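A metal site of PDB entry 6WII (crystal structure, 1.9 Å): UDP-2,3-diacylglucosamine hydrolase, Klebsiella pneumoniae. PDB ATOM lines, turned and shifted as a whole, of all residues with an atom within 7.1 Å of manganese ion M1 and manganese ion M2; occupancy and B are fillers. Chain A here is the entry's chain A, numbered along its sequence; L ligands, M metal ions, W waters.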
ATOM      1  N   ALA A   7       6.185  23.911  -2.596  1.00  0.00           N
ATOM      2  CA  ALA A   7       6.510  22.529  -2.236  1.00  0.00           C
ATOM      3  C   ALA A   7       5.202  21.791  -2.004  1.00  0.00           C
ATOM      4  O   ALA A   7       4.125  22.395  -1.887  1.00  0.00           O
ATOM      5  CB  ALA A   7       7.399  22.450  -1.002  1.00  0.00           C
ATOM      6  N   ASP A   8       5.307  20.463  -1.918  1.00  0.00           N
ATOM      7  CA  ASP A   8       4.196  19.647  -1.462  1.00  0.00           C
ATOM      8  C   ASP A   8       2.948  19.828  -2.338  1.00  0.00           C
ATOM      9  O   ASP A   8       1.821  19.933  -1.837  1.00  0.00           O
ATOM     10  CB  ASP A   8       3.887  19.935   0.000  1.00  0.00           C
ATOM     11  CG  ASP A   8       5.081  19.647   0.878  1.00  0.00           C
ATOM     12  OD1 ASP A   8       5.507  18.472   0.913  1.00  0.00           O
ATOM     13  OD2 ASP A   8       5.615  20.579   1.487  1.00  0.00           O
ATOM     14  N   LEU A   9       3.163  19.859  -3.643  1.00  0.00           N
ATOM     15  CA  LEU A   9       2.050  19.808  -4.581  1.00  0.00           C
ATOM     16  C   LEU A   9       1.467  18.402  -4.677  1.00  0.00           C
ATOM     17  O   LEU A   9       0.250  18.248  -4.879  1.00  0.00           O
ATOM     18  CB  LEU A   9       2.500  20.284  -5.960  1.00  0.00           C
ATOM     19  CG  LEU A   9       2.804  21.787  -6.022  1.00  0.00           C
ATOM     20  CD1 LEU A   9       4.231  22.121  -5.593  1.00  0.00           C
ATOM     21  CD2 LEU A   9       2.551  22.257  -7.436  1.00  0.00           C
ATOM     22  N   HIS A  10       2.306  17.370  -4.553  1.00  0.00           N
ATOM     23  CA  HIS A  10       1.867  15.971  -4.671  1.00  0.00           C
ATOM     24  C   HIS A  10       1.041  15.744  -5.930  1.00  0.00           C
ATOM     25  O   HIS A  10      -0.045  15.137  -5.901  1.00  0.00           O
ATOM     26  CB  HIS A  10       1.080  15.532  -3.428  1.00  0.00           C
ATOM     27  CG  HIS A  10       1.858  15.670  -2.152  1.00  0.00           C
ATOM     28  ND1 HIS A  10       2.527  14.616  -1.580  1.00  0.00           N
ATOM     29  CD2 HIS A  10       2.075  16.741  -1.358  1.00  0.00           C
ATOM     30  CE1 HIS A  10       3.129  15.027  -0.475  1.00  0.00           C
ATOM     31  NE2 HIS A  10       2.862  16.313  -0.322  1.00  0.00           N
ATOM     32  N   LEU A  39      10.650  22.940  -3.435  1.00  0.00           N
ATOM     33  CA  LEU A  39      11.293  22.301  -2.275  1.00  0.00           C
ATOM     34  C   LEU A  39      10.725  20.920  -1.973  1.00  0.00           C
ATOM     35  O   LEU A  39      10.426  20.615  -0.818  1.00  0.00           O
ATOM     36  CB  LEU A  39      11.168  23.215  -1.051  1.00  0.00           C
ATOM     37  CG  LEU A  39      11.743  24.626  -1.192  1.00  0.00           C
ATOM     38  CD1 LEU A  39      11.802  25.354   0.181  1.00  0.00           C
ATOM     39  CD2 LEU A  39      13.129  24.608  -1.859  1.00  0.00           C
ATOM     40  N   GLY A  40      10.564  20.094  -2.998  1.00  0.00           N
ATOM     41  CA  GLY A  40      10.265  18.687  -2.802  1.00  0.00           C
ATOM     42  C   GLY A  40       8.780  18.369  -2.813  1.00  0.00           C
ATOM     43  O   GLY A  40       7.917  19.231  -2.606  1.00  0.00           O
ATOM     44  N   ASP A  41       8.493  17.092  -3.062  1.00  0.00           N
ATOM     45  CA  ASP A  41       7.121  16.583  -3.140  1.00  0.00           C
ATOM     46  C   ASP A  41       6.349  17.316  -4.214  1.00  0.00           C
ATOM     47  O   ASP A  41       5.180  17.689  -4.053  1.00  0.00           O
ATOM     48  CB  ASP A  41       6.406  16.659  -1.782  1.00  0.00           C
ATOM     49  CG  ASP A  41       6.899  15.603  -0.810  1.00  0.00           C
ATOM     50  OD1 ASP A  41       7.810  14.820  -1.190  1.00  0.00           O
ATOM     51  OD2 ASP A  41       6.392  15.545   0.340  1.00  0.00           O
ATOM     52  N   GLU A  44       3.402  13.143  -6.274  1.00  0.00           N
ATOM     53  CA  GLU A  44       2.945  12.231  -5.234  1.00  0.00           C
ATOM     54  C   GLU A  44       3.790  10.969  -5.187  1.00  0.00           C
ATOM     55  O   GLU A  44       3.919  10.332  -4.121  1.00  0.00           O
ATOM     56  CB  GLU A  44       1.472  11.886  -5.465  1.00  0.00           C
ATOM     57  CG  GLU A  44       0.884  10.782  -4.552  1.00  0.00           C
ATOM     58  CD  GLU A  44       0.956  11.091  -3.070  1.00  0.00           C
ATOM     59  OE1 GLU A  44       1.233  12.248  -2.683  1.00  0.00           O
ATOM     60  OE2 GLU A  44       0.726  10.154  -2.264  1.00  0.00           O
ATOM     61  N   GLY A  78      11.863  15.716  -2.350  1.00  0.00           N
ATOM     62  CA  GLY A  78      11.046  15.444  -1.190  1.00  0.00           C
ATOM     63  C   GLY A  78      11.110  13.973  -0.808  1.00  0.00           C
ATOM     64  O   GLY A  78      11.821  13.175  -1.412  1.00  0.00           O
ATOM     65  N   ASN A  79      10.346  13.629   0.220  1.00  0.00           N
ATOM     66  CA  ASN A  79      10.241  12.220   0.624  1.00  0.00           C
ATOM     67  C   ASN A  79       9.484  11.390  -0.402  1.00  0.00           C
ATOM     68  O   ASN A  79       9.694  10.176  -0.475  1.00  0.00           O
ATOM     69  CB  ASN A  79       9.588  12.106   1.991  1.00  0.00           C
ATOM     70  CG  ASN A  79       8.216  12.750   2.030  1.00  0.00           C
ATOM     71  OD1 ASN A  79       8.087  13.962   1.947  1.00  0.00           O
ATOM     72  ND2 ASN A  79       7.166  11.928   2.183  1.00  0.00           N
ATOM     73  N   ARG A  80       8.610  12.008  -1.193  1.00  0.00           N
ATOM     74  CA  ARG A  80       7.856  11.245  -2.195  1.00  0.00           C
ATOM     75  C   ARG A  80       8.609  11.101  -3.501  1.00  0.00           C
ATOM     76  O   ARG A  80       8.465  10.064  -4.176  1.00  0.00           O
ATOM     77  CB  ARG A  80       6.508  11.906  -2.490  1.00  0.00           C
ATOM     78  CG  ARG A  80       5.632  12.143  -1.293  1.00  0.00           C
ATOM     79  CD  ARG A  80       5.293  10.853  -0.563  1.00  0.00           C
ATOM     80  NE  ARG A  80       4.440  10.008  -1.399  1.00  0.00           N
ATOM     81  CZ  ARG A  80       3.858   8.898  -0.970  1.00  0.00           C
ATOM     82  NH1 ARG A  80       4.015   8.500   0.294  1.00  0.00           N
ATOM     83  NH2 ARG A  80       3.095   8.181  -1.788  1.00  0.00           N
ATOM     84  N   HIS A 114      13.736  20.458   1.992  1.00  0.00           N
ATOM     85  CA  HIS A 114      12.376  19.936   1.984  1.00  0.00           C
ATOM     86  C   HIS A 114      11.759  19.985   3.370  1.00  0.00           C
ATOM     87  O   HIS A 114      10.591  20.358   3.531  1.00  0.00           O
ATOM     88  CB  HIS A 114      12.329  18.491   1.452  1.00  0.00           C
ATOM     89  CG  HIS A 114      10.951  17.936   1.446  1.00  0.00           C
ATOM     90  ND1 HIS A 114       9.911  18.535   0.775  1.00  0.00           N
ATOM     91  CD2 HIS A 114      10.411  16.853   2.070  1.00  0.00           C
ATOM     92  CE1 HIS A 114       8.799  17.834   0.956  1.00  0.00           C
ATOM     93  NE2 HIS A 114       9.082  16.815   1.746  1.00  0.00           N
ATOM     94  N   GLY A 115      12.515  19.608   4.392  1.00  0.00           N
ATOM     95  CA  GLY A 115      12.052  19.664   5.766  1.00  0.00           C
ATOM     96  C   GLY A 115      11.953  18.330   6.465  1.00  0.00           C
ATOM     97  O   GLY A 115      11.908  18.309   7.699  1.00  0.00           O
ATOM     98  N   ASP A 116      11.914  17.214   5.724  1.00  0.00           N
ATOM     99  CA  ASP A 116      11.733  15.928   6.401  1.00  0.00           C
ATOM    100  C   ASP A 116      12.921  15.588   7.278  1.00  0.00           C
ATOM    101  O   ASP A 116      12.757  14.892   8.297  1.00  0.00           O
ATOM    102  CB  ASP A 116      11.479  14.805   5.386  1.00  0.00           C
ATOM    103  CG  ASP A 116      12.606  14.644   4.390  1.00  0.00           C
ATOM    104  OD1 ASP A 116      13.055  15.650   3.800  1.00  0.00           O
ATOM    105  OD2 ASP A 116      13.060  13.505   4.198  1.00  0.00           O
ATOM    106  N   TYR A 125      10.920   6.830  10.347  1.00  0.00           N
ATOM    107  CA  TYR A 125      11.030   7.438   9.026  1.00  0.00           C
ATOM    108  C   TYR A 125      12.482   7.676   8.646  1.00  0.00           C
ATOM    109  O   TYR A 125      12.876   7.405   7.506  1.00  0.00           O
ATOM    110  CB  TYR A 125      10.266   8.764   8.951  1.00  0.00           C
ATOM    111  CG  TYR A 125      10.651   9.507   7.692  1.00  0.00           C
ATOM    112  CD1 TYR A 125      10.338   8.985   6.454  1.00  0.00           C
ATOM    113  CD2 TYR A 125      11.399  10.672   7.737  1.00  0.00           C
ATOM    114  CE1 TYR A 125      10.707   9.627   5.285  1.00  0.00           C
ATOM    115  CE2 TYR A 125      11.777  11.325   6.571  1.00  0.00           C
ATOM    116  CZ  TYR A 125      11.420  10.794   5.358  1.00  0.00           C
ATOM    117  OH  TYR A 125      11.791  11.426   4.187  1.00  0.00           O
ATOM    118  N   ILE A 171       1.421  13.968   9.630  1.00  0.00           N
ATOM    119  CA  ILE A 171       2.839  14.169   9.372  1.00  0.00           C
ATOM    120  C   ILE A 171       3.493  14.653  10.653  1.00  0.00           C
ATOM    121  O   ILE A 171       3.054  15.652  11.249  1.00  0.00           O
ATOM    122  CB  ILE A 171       3.062  15.164   8.217  1.00  0.00           C
ATOM    123  CG1 ILE A 171       2.410  14.661   6.932  1.00  0.00           C
ATOM    124  CG2 ILE A 171       4.552  15.415   7.999  1.00  0.00           C
ATOM    125  CD1 ILE A 171       2.395  15.679   5.805  1.00  0.00           C
ATOM    126  N   GLY A 194       9.226  22.836   3.457  1.00  0.00           N
ATOM    127  CA  GLY A 194       7.887  22.323   3.362  1.00  0.00           C
ATOM    128  C   GLY A 194       7.754  21.072   4.196  1.00  0.00           C
ATOM    129  O   GLY A 194       8.130  21.069   5.373  1.00  0.00           O
ATOM    130  N   HIS A 195       7.219  20.020   3.573  1.00  0.00           N
ATOM    131  CA  HIS A 195       7.043  18.689   4.170  1.00  0.00           C
ATOM    132  C   HIS A 195       5.963  18.606   5.234  1.00  0.00           C
ATOM    133  O   HIS A 195       5.150  17.668   5.197  1.00  0.00           O
ATOM    134  CB  HIS A 195       8.327  18.139   4.809  1.00  0.00           C
ATOM    135  CG  HIS A 195       8.155  16.723   5.265  1.00  0.00           C
ATOM    136  ND1 HIS A 195       7.916  15.686   4.393  1.00  0.00           N
ATOM    137  CD2 HIS A 195       8.092  16.176   6.512  1.00  0.00           C
ATOM    138  CE1 HIS A 195       7.767  14.558   5.066  1.00  0.00           C
ATOM    139  NE2 HIS A 195       7.856  14.834   6.358  1.00  0.00           N
ATOM    140  N   THR A 196       5.954  19.519   6.205  1.00  0.00           N
ATOM    141  CA  THR A 196       5.073  19.325   7.353  1.00  0.00           C
ATOM    142  C   THR A 196       3.643  19.755   7.103  1.00  0.00           C
ATOM    143  O   THR A 196       2.788  19.481   7.939  1.00  0.00           O
ATOM    144  CB  THR A 196       5.607  20.076   8.572  1.00  0.00           C
ATOM    145  OG1 THR A 196       5.648  21.469   8.270  1.00  0.00           O
ATOM    146  CG2 THR A 196       7.006  19.570   8.936  1.00  0.00           C
ATOM    147  N   HIS A 197       3.364  20.449   5.989  1.00  0.00           N
ATOM    148  CA  HIS A 197       2.001  20.844   5.637  1.00  0.00           C
ATOM    149  C   HIS A 197       1.365  21.768   6.677  1.00  0.00           C
ATOM    150  O   HIS A 197       0.149  21.790   6.831  1.00  0.00           O
ATOM    151  CB  HIS A 197       1.110  19.618   5.417  1.00  0.00           C
ATOM    152  CG  HIS A 197       1.524  18.756   4.270  1.00  0.00           C
ATOM    153  ND1 HIS A 197       0.699  17.784   3.731  1.00  0.00           N
ATOM    154  CD2 HIS A 197       2.676  18.717   3.549  1.00  0.00           C
ATOM    155  CE1 HIS A 197       1.329  17.189   2.728  1.00  0.00           C
ATOM    156  NE2 HIS A 197       2.534  17.733   2.607  1.00  0.00           N
ATOM    157  N   ALA A 218       0.848  22.621   1.730  1.00  0.00           N
ATOM    158  CA  ALA A 218       0.558  21.667   0.673  1.00  0.00           C
ATOM    159  C   ALA A 218      -0.574  22.212  -0.185  1.00  0.00           C
ATOM    160  O   ALA A 218      -1.396  23.009   0.271  1.00  0.00           O
ATOM    161  CB  ALA A 218       0.172  20.307   1.269  1.00  0.00           C
HETATM  162  C1  LIG L   1       7.303   7.429  -1.883  1.00  0.00           C
HETATM  163  C2  LIG L   1       6.714   6.724   0.336  1.00  0.00           C
HETATM  164  C3  LIG L   1       6.128   5.351  -1.543  1.00  0.00           C
HETATM  165  C4  LIG L   1       7.368   9.299   4.717  1.00  0.00           C
HETATM  166  C5  LIG L   1       6.393  11.183   6.079  1.00  0.00           C
HETATM  167  C6  LIG L   1       7.394  12.023   8.207  1.00  0.00           C
HETATM  168  C7  LIG L   1      12.668   3.268  -3.871  1.00  0.00           C
HETATM  169  C8  LIG L   1      11.431   2.724  -3.662  1.00  0.00           C
HETATM  170  C9  LIG L   1       9.025   2.781  -4.294  1.00  0.00           C
HETATM  171  C10 LIG L   1       7.926   3.696  -3.786  1.00  0.00           C
HETATM  172  C11 LIG L   1       9.311   5.636  -4.263  1.00  0.00           C
HETATM  173  C12 LIG L   1      10.410   4.721  -4.771  1.00  0.00           C
HETATM  174  C13 LIG L   1       6.718   6.288  -2.387  1.00  0.00           C
HETATM  175  C14 LIG L   1       7.286   7.651  -0.522  1.00  0.00           C
HETATM  176  C15 LIG L   1       6.152   5.566  -0.179  1.00  0.00           C
HETATM  177  C16 LIG L   1       7.104   8.108   2.534  1.00  0.00           C
HETATM  178  C17 LIG L   1       6.258   9.701   5.693  1.00  0.00           C
HETATM  179  C18 LIG L   1       7.690  11.385   6.856  1.00  0.00           C
HETATM  180  C19 LIG L   1      11.253   1.470  -3.091  1.00  0.00           C
HETATM  181  C20 LIG L   1      12.359   0.770  -2.710  1.00  0.00           C
HETATM  182  C21 LIG L   1      13.625   1.292  -2.900  1.00  0.00           C
HETATM  183  C22 LIG L   1      13.774   2.544  -3.475  1.00  0.00           C
HETATM  184  C23 LIG L   1      12.152  -0.610  -2.086  1.00  0.00           C
HETATM  185  F1  LIG L   1      11.538  -1.410  -2.986  1.00  0.00           F
HETATM  186  F2  LIG L   1      11.358  -0.478  -0.994  1.00  0.00           F
HETATM  187  F3  LIG L   1      13.356  -1.136  -1.761  1.00  0.00           F
HETATM  188  N1  LIG L   1      10.276   3.456  -4.073  1.00  0.00           N
HETATM  189  N2  LIG L   1       8.034   4.994  -4.460  1.00  0.00           N
HETATM  190  N3  LIG L   1       6.648   6.927   1.770  1.00  0.00           N
HETATM  191  N4  LIG L   1       6.928   8.137   3.969  1.00  0.00           N
HETATM  192  N5  LIG L   1       8.160  13.174   8.643  1.00  0.00           N
HETATM  193  O1  LIG L   1       6.992   7.233  -4.934  1.00  0.00           O
HETATM  194  O2  LIG L   1       5.488   5.401  -4.594  1.00  0.00           O
HETATM  195  O3  LIG L   1       7.626   9.041   2.040  1.00  0.00           O
HETATM  196  O4  LIG L   1       6.539  11.582   8.906  1.00  0.00           O
HETATM  197  O5  LIG L   1       7.881  13.774   9.886  1.00  0.00           O
HETATM  198  S1  LIG L   1       6.744   6.014  -4.159  1.00  0.00           S
HETATM  199 CL1  LIG L   1      15.359   3.295  -3.743  1.00  0.00          CL
HETATM  200 MN    MN M   1       4.282  16.902   1.301  1.00  0.00          MN
HETATM  201 MN    MN M   2       7.268  15.653   2.332  1.00  0.00          MN
HETATM  202  O   HOH W   1       4.599  13.505   2.382  1.00  0.00           O
HETATM  203  O   HOH W   2       5.172  16.013   2.696  1.00  0.00           O
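A ring nitrogen (NE2) of His 195 lies within hydrogen-bond range of a nitrogen (N5) of the ligand (2.8 Å). An oxygen (O3) of the ligand sits at hydrogen-bond distance from the side-chain amide nitrogen of Asn 79.
O of Leu 39 sits at hydrogen-bond distance from ND1 of His 114, at 2.7 Å. O of Asp 41 sits at hydrogen-bond distance from N of Leu 9 (3.0 Å). The backbone carbonyl oxygen (O) of His 114 sits at hydrogen-bond distance from the backbone NH (N) of Gly 194 (2.8 Å). The side-chain carboxylate (OD1) of Asp 41 lies within hydrogen-bond range of the backbone NH (N) of Arg 80 (2.9 Å). A ring nitrogen (ND1) of His 10 lies within hydrogen-bond range of the side-chain carboxylate (OE1) of Glu 44 (2.9 Å). O of Gly 40 lies within hydrogen-bond range of N of Asp 8 (3.0 Å). The backbone NH (N) of His 195 is in hydrogen-bond range of the side-chain carboxylate (OD2) of Asp 8 (2.7 Å).
Four residues have an atom within 4 Å of manganese ion M1: Asp 8, His 10, Asp 41 and His 197. The nearest printed residue that does not touch manganese ion M1 is His 195 (4.1 Å).
Within 4 Å of manganese ion M2: Asp 8, Asp 41, Asn 79, His 114 and His 195. The nearest printed residue that does not touch manganese ion M2 is His 10 (5.0 Å).
Manganese ion M1 is bound by water W2, the side-chain carboxylate of Asp 8, a ring nitrogen (NE2) of His 10, a ring nitrogen (NE2) of His 197 and the side-chain carboxylate of Asp 41. Manganese ion M1 has five donor atoms within binding distance.
Manganese ion M2 is bound by the side-chain amide oxygen of Asn 79 (1.9 Å), water W2 (2.2 Å), a ring nitrogen (ND1) of His 195 (2.2 Å), the side-chain carboxylate of Asp 41 (2.2 Å) and a ring nitrogen (NE2) of His 114 (2.2 Å).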
